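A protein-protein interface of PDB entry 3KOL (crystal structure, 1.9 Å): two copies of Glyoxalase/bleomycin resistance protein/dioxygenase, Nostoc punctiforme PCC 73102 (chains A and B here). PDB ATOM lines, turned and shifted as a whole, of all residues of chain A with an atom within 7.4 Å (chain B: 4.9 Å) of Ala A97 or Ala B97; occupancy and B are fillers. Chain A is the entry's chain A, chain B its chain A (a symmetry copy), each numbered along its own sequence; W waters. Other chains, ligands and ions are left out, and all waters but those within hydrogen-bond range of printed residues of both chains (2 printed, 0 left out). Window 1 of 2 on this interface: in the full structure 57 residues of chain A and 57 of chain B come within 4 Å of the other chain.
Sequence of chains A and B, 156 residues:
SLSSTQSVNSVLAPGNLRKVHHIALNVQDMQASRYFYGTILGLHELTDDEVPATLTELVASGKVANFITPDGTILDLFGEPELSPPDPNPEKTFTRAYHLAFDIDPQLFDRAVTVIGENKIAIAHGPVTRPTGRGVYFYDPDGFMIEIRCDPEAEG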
ATOM      1  N   ILE A  23      -2.553   2.047  32.291  1.00  0.00           N
ATOM      2  CA  ILE A  23      -1.986   3.380  32.144  1.00  0.00           C
ATOM      3  C   ILE A  23      -2.881   3.989  31.073  1.00  0.00           C
ATOM      4  O   ILE A  23      -3.122   3.372  30.034  1.00  0.00           O
ATOM      5  CB  ILE A  23      -0.519   3.368  31.661  1.00  0.00           C
ATOM      6  CG1 ILE A  23      -0.048   4.810  31.446  1.00  0.00           C
ATOM      7  CG2 ILE A  23      -0.381   2.565  30.388  1.00  0.00           C
ATOM      8  CD1 ILE A  23       1.421   4.938  31.167  1.00  0.00           C
ATOM      9  N   ALA A  24      -3.401   5.178  31.335  1.00  0.00           N
ATOM     10  CA  ALA A  24      -4.292   5.827  30.389  1.00  0.00           C
ATOM     11  C   ALA A  24      -3.624   6.999  29.699  1.00  0.00           C
ATOM     12  O   ALA A  24      -2.882   7.763  30.316  1.00  0.00           O
ATOM     13  CB  ALA A  24      -5.554   6.298  31.105  1.00  0.00           C
ATOM     14  N   LEU A  25      -3.891   7.120  28.405  1.00  0.00           N
ATOM     15  CA  LEU A  25      -3.349   8.194  27.596  1.00  0.00           C
ATOM     16  C   LEU A  25      -4.504   8.902  26.902  1.00  0.00           C
ATOM     17  O   LEU A  25      -5.506   8.275  26.562  1.00  0.00           O
ATOM     18  CB  LEU A  25      -2.401   7.648  26.518  1.00  0.00           C
ATOM     19  CG  LEU A  25      -1.233   6.720  26.878  1.00  0.00           C
ATOM     20  CD1 LEU A  25      -0.441   6.395  25.608  1.00  0.00           C
ATOM     21  CD2 LEU A  25      -0.326   7.380  27.901  1.00  0.00           C
ATOM     22  N   ASN A  26      -4.369  10.212  26.720  1.00  0.00           N
ATOM     23  CA  ASN A  26      -5.371  10.991  25.999  1.00  0.00           C
ATOM     24  C   ASN A  26      -4.777  11.167  24.608  1.00  0.00           C
ATOM     25  O   ASN A  26      -3.620  11.568  24.479  1.00  0.00           O
ATOM     26  CB  ASN A  26      -5.573  12.367  26.628  1.00  0.00           C
ATOM     27  CG  ASN A  26      -6.281  12.296  27.953  1.00  0.00           C
ATOM     28  OD1 ASN A  26      -7.129  11.428  28.164  1.00  0.00           O
ATOM     29  ND2 ASN A  26      -5.946  13.212  28.857  1.00  0.00           N
ATOM     30  N   PRO A  86       0.998  19.170  25.964  1.00  0.00           N
ATOM     31  CA  PRO A  86       1.572  20.190  26.848  1.00  0.00           C
ATOM     32  C   PRO A  86       2.403  21.204  26.059  1.00  0.00           C
ATOM     33  O   PRO A  86       2.518  22.366  26.448  1.00  0.00           O
ATOM     34  CB  PRO A  86       2.398  19.368  27.840  1.00  0.00           C
ATOM     35  CG  PRO A  86       2.713  18.113  27.088  1.00  0.00           C
ATOM     36  CD  PRO A  86       1.421  17.821  26.371  1.00  0.00           C
ATOM     37  N   THR A  93      10.412  19.098  27.694  1.00  0.00           N
ATOM     38  CA  THR A  93      10.096  18.283  28.868  1.00  0.00           C
ATOM     39  C   THR A  93       9.418  19.020  30.027  1.00  0.00           C
ATOM     40  O   THR A  93       9.592  20.227  30.208  1.00  0.00           O
ATOM     41  CB  THR A  93      11.366  17.594  29.408  1.00  0.00           C
ATOM     42  OG1 THR A  93      12.343  18.586  29.746  1.00  0.00           O
ATOM     43  CG2 THR A  93      11.952  16.652  28.352  1.00  0.00           C
ATOM     44  N   PHE A  94       8.653  18.266  30.815  1.00  0.00           N
ATOM     45  CA  PHE A  94       7.919  18.795  31.965  1.00  0.00           C
ATOM     46  C   PHE A  94       7.944  17.754  33.074  1.00  0.00           C
ATOM     47  O   PHE A  94       8.435  16.645  32.878  1.00  0.00           O
ATOM     48  CB  PHE A  94       6.449  19.032  31.607  1.00  0.00           C
ATOM     49  CG  PHE A  94       6.228  20.020  30.497  1.00  0.00           C
ATOM     50  CD1 PHE A  94       6.312  21.388  30.735  1.00  0.00           C
ATOM     51  CD2 PHE A  94       5.915  19.581  29.215  1.00  0.00           C
ATOM     52  CE1 PHE A  94       6.081  22.311  29.707  1.00  0.00           C
ATOM     53  CE2 PHE A  94       5.683  20.493  28.184  1.00  0.00           C
ATOM     54  CZ  PHE A  94       5.767  21.861  28.433  1.00  0.00           C
ATOM     55  N   THR A  95       7.402  18.112  34.234  1.00  0.00           N
ATOM     56  CA  THR A  95       7.308  17.159  35.327  1.00  0.00           C
ATOM     57  C   THR A  95       6.136  16.258  34.932  1.00  0.00           C
ATOM     58  O   THR A  95       5.490  16.502  33.905  1.00  0.00           O
ATOM     59  CB  THR A  95       6.998  17.845  36.675  1.00  0.00           C
ATOM     60  OG1 THR A  95       5.841  18.676  36.538  1.00  0.00           O
ATOM     61  CG2 THR A  95       8.186  18.686  37.129  1.00  0.00           C
ATOM     62  N   ARG A  96       5.869  15.237  35.745  1.00  0.00           N
ATOM     63  CA  ARG A  96       4.805  14.255  35.507  1.00  0.00           C
ATOM     64  C   ARG A  96       5.293  13.153  34.552  1.00  0.00           C
ATOM     65  O   ARG A  96       6.486  12.855  34.532  1.00  0.00           O
ATOM     66  CB  ARG A  96       3.524  14.936  34.995  1.00  0.00           C
ATOM     67  CG  ARG A  96       2.912  15.907  36.021  1.00  0.00           C
ATOM     68  CD  ARG A  96       1.688  16.646  35.476  1.00  0.00           C
ATOM     69  NE  ARG A  96       1.269  17.723  36.372  1.00  0.00           N
ATOM     70  CZ  ARG A  96       0.352  18.641  36.076  1.00  0.00           C
ATOM     71  NH1 ARG A  96      -0.261  18.625  34.896  1.00  0.00           N
ATOM     72  NH2 ARG A  96       0.054  19.585  36.965  1.00  0.00           N
ATOM     73  N   ALA A  97       4.401  12.553  33.763  1.00  0.00           N
ATOM     74  CA  ALA A  97       4.791  11.444  32.877  1.00  0.00           C
ATOM     75  C   ALA A  97       5.952  11.737  31.930  1.00  0.00           C
ATOM     76  O   ALA A  97       5.935  12.719  31.191  1.00  0.00           O
ATOM     77  CB  ALA A  97       3.578  10.949  32.077  1.00  0.00           C
ATOM     78  N   TYR A  98       6.950  10.856  31.956  1.00  0.00           N
ATOM     79  CA  TYR A  98       8.160  10.976  31.137  1.00  0.00           C
ATOM     80  C   TYR A  98       8.108   9.975  29.980  1.00  0.00           C
ATOM     81  O   TYR A  98       8.104  10.368  28.819  1.00  0.00           O
ATOM     82  CB  TYR A  98       9.372  10.744  32.047  1.00  0.00           C
ATOM     83  CG  TYR A  98      10.740  10.696  31.400  1.00  0.00           C
ATOM     84  CD1 TYR A  98      10.966  11.193  30.117  1.00  0.00           C
ATOM     85  CD2 TYR A  98      11.825  10.170  32.105  1.00  0.00           C
ATOM     86  CE1 TYR A  98      12.245  11.162  29.551  1.00  0.00           C
ATOM     87  CE2 TYR A  98      13.098  10.139  31.552  1.00  0.00           C
ATOM     88  CZ  TYR A  98      13.301  10.636  30.278  1.00  0.00           C
ATOM     89  OH  TYR A  98      14.565  10.608  29.739  1.00  0.00           O
ATOM     90  N   HIS A  99       8.082   8.683  30.288  1.00  0.00           N
ATOM     91  CA  HIS A  99       7.967   7.684  29.231  1.00  0.00           C
ATOM     92  C   HIS A  99       7.393   6.374  29.732  1.00  0.00           C
ATOM     93  O   HIS A  99       7.309   6.131  30.936  1.00  0.00           O
ATOM     94  CB  HIS A  99       9.309   7.438  28.509  1.00  0.00           C
ATOM     95  CG  HIS A  99      10.377   6.815  29.355  1.00  0.00           C
ATOM     96  ND1 HIS A  99      11.224   7.556  30.152  1.00  0.00           N
ATOM     97  CD2 HIS A  99      10.787   5.528  29.468  1.00  0.00           C
ATOM     98  CE1 HIS A  99      12.113   6.754  30.712  1.00  0.00           C
ATOM     99  NE2 HIS A  99      11.870   5.519  30.315  1.00  0.00           N
ATOM    100  N   LEU A 100       6.961   5.551  28.789  1.00  0.00           N
ATOM    101  CA  LEU A 100       6.385   4.248  29.082  1.00  0.00           C
ATOM    102  C   LEU A 100       7.260   3.248  28.335  1.00  0.00           C
ATOM    103  O   LEU A 100       7.471   3.386  27.129  1.00  0.00           O
ATOM    104  CB  LEU A 100       4.941   4.180  28.565  1.00  0.00           C
ATOM    105  CG  LEU A 100       4.286   2.796  28.584  1.00  0.00           C
ATOM    106  CD1 LEU A 100       4.205   2.272  30.018  1.00  0.00           C
ATOM    107  CD2 LEU A 100       2.898   2.888  27.969  1.00  0.00           C
ATOM    108  N   ASP A 140       4.988   8.749  20.256  1.00  0.00           N
ATOM    109  CA  ASP A 140       3.744   8.242  19.684  1.00  0.00           C
ATOM    110  C   ASP A 140       3.106   9.425  18.954  1.00  0.00           C
ATOM    111  O   ASP A 140       3.653  10.530  18.990  1.00  0.00           O
ATOM    112  CB  ASP A 140       2.828   7.650  20.781  1.00  0.00           C
ATOM    113  CG  ASP A 140       2.062   8.701  21.586  1.00  0.00           C
ATOM    114  OD1 ASP A 140       2.288   9.922  21.435  1.00  0.00           O
ATOM    115  OD2 ASP A 140       1.212   8.282  22.400  1.00  0.00           O
ATOM    116  N   ASP A 142       0.942  11.578  19.585  1.00  0.00           N
ATOM    117  CA  ASP A 142       0.695  12.789  20.364  1.00  0.00           C
ATOM    118  C   ASP A 142       1.954  13.385  20.976  1.00  0.00           C
ATOM    119  O   ASP A 142       1.907  14.451  21.587  1.00  0.00           O
ATOM    120  CB  ASP A 142      -0.321  12.502  21.472  1.00  0.00           C
ATOM    121  CG  ASP A 142      -1.708  12.231  20.927  1.00  0.00           C
ATOM    122  OD1 ASP A 142      -2.363  13.197  20.483  1.00  0.00           O
ATOM    123  OD2 ASP A 142      -2.141  11.058  20.930  1.00  0.00           O
ATOM    124  N   PHE A 144       4.012  11.498  23.080  1.00  0.00           N
ATOM    125  CA  PHE A 144       4.350  10.803  24.324  1.00  0.00           C
ATOM    126  C   PHE A 144       5.463   9.808  24.009  1.00  0.00           C
ATOM    127  O   PHE A 144       5.342   9.002  23.085  1.00  0.00           O
ATOM    128  CB  PHE A 144       3.137  10.058  24.886  1.00  0.00           C
ATOM    129  CG  PHE A 144       3.414   9.352  26.180  1.00  0.00           C
ATOM    130  CD1 PHE A 144       3.799  10.071  27.305  1.00  0.00           C
ATOM    131  CD2 PHE A 144       3.318   7.967  26.271  1.00  0.00           C
ATOM    132  CE1 PHE A 144       4.089   9.422  28.505  1.00  0.00           C
ATOM    133  CE2 PHE A 144       3.604   7.304  27.466  1.00  0.00           C
ATOM    134  CZ  PHE A 144       3.991   8.032  28.584  1.00  0.00           C
ATOM    135  N   MET A 145       6.541   9.852  24.782  1.00  0.00           N
ATOM    136  CA  MET A 145       7.680   8.979  24.528  1.00  0.00           C
ATOM    137  C   MET A 145       7.519   7.521  24.938  1.00  0.00           C
ATOM    138  O   MET A 145       7.160   7.212  26.072  1.00  0.00           O
ATOM    139  CB  MET A 145       8.936   9.546  25.192  1.00  0.00           C
ATOM    140  CG  MET A 145      10.179   8.723  24.926  1.00  0.00           C
ATOM    141  SD  MET A 145      11.727   9.453  25.816  1.00  0.00           S
ATOM    142  CE  MET A 145      12.360  10.588  24.378  1.00  0.00           C
ATOM    143  N   ALA B  24       8.001   5.828  33.598  1.00  0.00           N
ATOM    144  CA  ALA B  24       8.865   6.824  34.207  1.00  0.00           C
ATOM    145  C   ALA B  24       8.156   8.152  34.385  1.00  0.00           C
ATOM    146  O   ALA B  24       7.394   8.588  33.522  1.00  0.00           O
ATOM    147  CB  ALA B  24      10.117   7.015  33.355  1.00  0.00           C
ATOM    148  N   LEU B  25       8.411   8.780  35.526  1.00  0.00           N
ATOM    149  CA  LEU B  25       7.830  10.068  35.851  1.00  0.00           C
ATOM    150  C   LEU B  25       8.958  11.027  36.203  1.00  0.00           C
ATOM    151  O   LEU B  25       9.977  10.616  36.756  1.00  0.00           O
ATOM    152  CB  LEU B  25       6.893   9.960  37.063  1.00  0.00           C
ATOM    153  CG  LEU B  25       5.757   8.929  37.104  1.00  0.00           C
ATOM    154  CD1 LEU B  25       4.967   9.105  38.405  1.00  0.00           C
ATOM    155  CD2 LEU B  25       4.837   9.105  35.910  1.00  0.00           C
ATOM    156  N   ASN B  26       8.781  12.299  35.857  1.00  0.00           N
ATOM    157  CA  ASN B  26       9.754  13.330  36.206  1.00  0.00           C
ATOM    158  C   ASN B  26       9.145  14.020  37.420  1.00  0.00           C
ATOM    159  O   ASN B  26       7.976  14.403  37.388  1.00  0.00           O
ATOM    160  CB  ASN B  26       9.917  14.354  35.086  1.00  0.00           C
ATOM    161  CG  ASN B  26      10.635  13.789  33.891  1.00  0.00           C
ATOM    162  OD1 ASN B  26      11.510  12.935  34.033  1.00  0.00           O
ATOM    163  ND2 ASN B  26      10.277  14.265  32.702  1.00  0.00           N
ATOM    164  N   THR B  95      -3.183  16.235  25.917  1.00  0.00           N
ATOM    165  CA  THR B  95      -3.053  14.932  25.286  1.00  0.00           C
ATOM    166  C   THR B  95      -1.855  14.297  25.996  1.00  0.00           C
ATOM    167  O   THR B  95      -1.224  14.945  26.840  1.00  0.00           O
ATOM    168  CB  THR B  95      -2.756  15.043  23.776  1.00  0.00           C
ATOM    169  OG1 THR B  95      -1.626  15.897  23.568  1.00  0.00           O
ATOM    170  CG2 THR B  95      -3.967  15.599  23.035  1.00  0.00           C
ATOM    171  N   ARG B  96      -1.551  13.047  25.648  1.00  0.00           N
ATOM    172  CA  ARG B  96      -0.459  12.272  26.246  1.00  0.00           C
ATOM    173  C   ARG B  96      -0.918  11.619  27.561  1.00  0.00           C
ATOM    174  O   ARG B  96      -2.101  11.316  27.704  1.00  0.00           O
ATOM    175  CB  ARG B  96       0.798  13.139  26.441  1.00  0.00           C
ATOM    176  CG  ARG B  96       1.384  13.647  25.112  1.00  0.00           C
ATOM    177  CD  ARG B  96       2.582  14.579  25.315  1.00  0.00           C
ATOM    178  NE  ARG B  96       2.972  15.230  24.065  1.00  0.00           N
ATOM    179  CZ  ARG B  96       3.858  16.218  23.970  1.00  0.00           C
ATOM    180  NH1 ARG B  96       4.464  16.686  25.057  1.00  0.00           N
ATOM    181  NH2 ARG B  96       4.133  16.745  22.780  1.00  0.00           N
ATOM    182  N   ALA B  97      -0.012  11.406  28.516  1.00  0.00           N
ATOM    183  CA  ALA B  97      -0.374  10.723  29.770  1.00  0.00           C
ATOM    184  C   ALA B  97      -1.549  11.328  30.533  1.00  0.00           C
ATOM    185  O   ALA B  97      -1.567  12.521  30.826  1.00  0.00           O
ATOM    186  CB  ALA B  97       0.849  10.620  30.692  1.00  0.00           C
ATOM    187  N   TYR B  98      -2.519  10.477  30.861  1.00  0.00           N
ATOM    188  CA  TYR B  98      -3.737  10.871  31.575  1.00  0.00           C
ATOM    189  C   TYR B  98      -3.661  10.408  33.032  1.00  0.00           C
ATOM    190  O   TYR B  98      -3.677  11.226  33.945  1.00  0.00           O
ATOM    191  CB  TYR B  98      -4.936  10.262  30.838  1.00  0.00           C
ATOM    192  CG  TYR B  98      -6.306  10.430  31.460  1.00  0.00           C
ATOM    193  CD1 TYR B  98      -6.556  11.384  32.446  1.00  0.00           C
ATOM    194  CD2 TYR B  98      -7.368   9.635  31.026  1.00  0.00           C
ATOM    195  CE1 TYR B  98      -7.836  11.537  32.987  1.00  0.00           C
ATOM    196  CE2 TYR B  98      -8.643   9.784  31.554  1.00  0.00           C
ATOM    197  CZ  TYR B  98      -8.870  10.735  32.532  1.00  0.00           C
ATOM    198  OH  TYR B  98     -10.136  10.882  33.046  1.00  0.00           O
ATOM    199  N   HIS B  99      -3.593   9.101  33.257  1.00  0.00           N
ATOM    200  CA  HIS B  99      -3.454   8.601  34.621  1.00  0.00           C
ATOM    201  C   HIS B  99      -2.835   7.219  34.671  1.00  0.00           C
ATOM    202  O   HIS B  99      -2.736   6.524  33.659  1.00  0.00           O
ATOM    203  CB  HIS B  99      -4.791   8.618  35.390  1.00  0.00           C
ATOM    204  CG  HIS B  99      -5.834   7.679  34.864  1.00  0.00           C
ATOM    205  ND1 HIS B  99      -6.698   8.020  33.845  1.00  0.00           N
ATOM    206  CD2 HIS B  99      -6.203   6.439  35.268  1.00  0.00           C
ATOM    207  CE1 HIS B  99      -7.558   7.035  33.651  1.00  0.00           C
ATOM    208  NE2 HIS B  99      -7.280   6.064  34.500  1.00  0.00           N
ATOM    209  N   PHE B 144       0.340  14.649  38.751  1.00  0.00           N
ATOM    210  CA  PHE B 144       0.033  13.510  37.883  1.00  0.00           C
ATOM    211  C   PHE B 144      -1.050  12.685  38.571  1.00  0.00           C
ATOM    212  O   PHE B 144      -0.910  12.312  39.737  1.00  0.00           O
ATOM    213  CB  PHE B 144       1.272  12.643  37.652  1.00  0.00           C
ATOM    214  CG  PHE B 144       1.025  11.476  36.741  1.00  0.00           C
ATOM    215  CD1 PHE B 144       0.625  11.683  35.426  1.00  0.00           C
ATOM    216  CD2 PHE B 144       1.166  10.171  37.202  1.00  0.00           C
ATOM    217  CE1 PHE B 144       0.364  10.605  34.580  1.00  0.00           C
ATOM    218  CE2 PHE B 144       0.908   9.083  36.365  1.00  0.00           C
ATOM    219  CZ  PHE B 144       0.505   9.301  35.053  1.00  0.00           C
HETATM  220  O   HOH W   1       3.326  16.870  19.944  1.00  0.00           O
HETATM  221  O   HOH W   2      -1.615  15.794  20.759  1.00  0.00           O
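The backbone carbonyl oxygen (O) of Ala A24 is in hydrogen-bond range of the backbone NH (N) of Tyr B98 (2.8 Å).
The backbone carbonyl oxygen (O) of His B99 sits at hydrogen-bond distance from the backbone NH (N) of Ala A24 (2.8 Å).
The backbone NH (N) of Asn A26 lies within hydrogen-bond range of the backbone carbonyl oxygen (O) of Arg B96.
The backbone carbonyl oxygen (O) of Phe A94 is in hydrogen-bond range of the side-chain amide nitrogen (ND2) of Asn B26.
The backbone carbonyl oxygen of Arg A96 lies within hydrogen-bond range of the backbone NH of Asn B26.
O of Ala B24 sits at hydrogen-bond distance from N of Tyr A98 (2.8 Å).
The backbone carbonyl oxygen (O) of His A99 lies within hydrogen-bond range of the backbone NH (N) of Ala B24 (2.8 Å).
O of Asp A142 sits at hydrogen-bond distance from NE of Arg B96 (2.8 Å).
The side-chain carboxylate of Asp A140 sits at hydrogen-bond distance from the backbone NH of Asp A142 (2.8 Å).
The side-chain carboxylate of Asp A140 is in hydrogen-bond range of the backbone NH of Phe A144, 2.9 Å away.
Among the printed residues, merely in contact across the chains: Pro A86 with Arg B96, Ala A97 with Ala B97, Arg A96 with Leu B25, Leu A25 with Arg B96, Tyr A98 with Asn B26, Asn A26 with Tyr B98, Asn A26 with Thr B95, Thr A95 with Asn B26, Ile A23 with His B99, Asp A142 with Thr B95, Ala A97 with Ala B24, Ala A24 with Ala B97, Leu A25 with Ala B97, Ala A97 with Leu B25, Pro A86 with Thr B95, Arg A96 with Phe B144 and Phe A144 with Arg B96.
Of the printed residues of chain B, Ala A97 touches Ala B24, Leu B25 and Ala B97.
Of chain A, only Ala A24, Leu A25 and Ala A97 come within 4 Å of Ala B97.
Printed residues of chain A within 4 Å of Tyr B98: Ala A24 and Asn A26.
Printed residues of chain A within 4 Å of Arg B96: Leu A25, Asn A26, Pro A86, Asp A142 and Phe A144.
Printed residues of chain B within 4 Å of Leu A25: Arg B96 and Ala B97.
Of the printed residues of chain A, His B99 touches Ile A23 and Ala A24.
The nearest residue of chain B that does not touch Ala A97 is Phe B144 (4.1 Å).
The nearest printed residue of chain B that does not touch Ala A24 is Arg B96 (4.5 Å).
Of the 17 printed residues of chain A, 13 touch a printed residue of chain B.
Among the printed residues, no Asp or Glu carboxylate lies within 4 Å of a Lys or Arg side-chain nitrogen of the other chain.
Ala A24 touches His B99, and with the chains exchanged His A99 touches Ala B24.
Leu A25 touches Arg B96, and with the chains exchanged Arg A96 touches Leu B25.
Asn A26 touches Arg B96, and with the chains exchanged Arg A96 touches Asn B26.
Ala B97 touches its own counterpart, Ala A97.
Positions printed for both chains: 24, 25, 26, 95, 96, 97, 98, 99 and 144.
Water W2 lies within hydrogen-bond range of the side-chain carboxylate (OD1) of Asp A142 (2.7 Å) and the side-chain hydroxyl (OG1) of Thr B95 (2.8 Å).
Water W1 lies within hydrogen-bond range of NH2 of Arg B96 (3.0 Å) and O of Asp A142 (3.3 Å).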
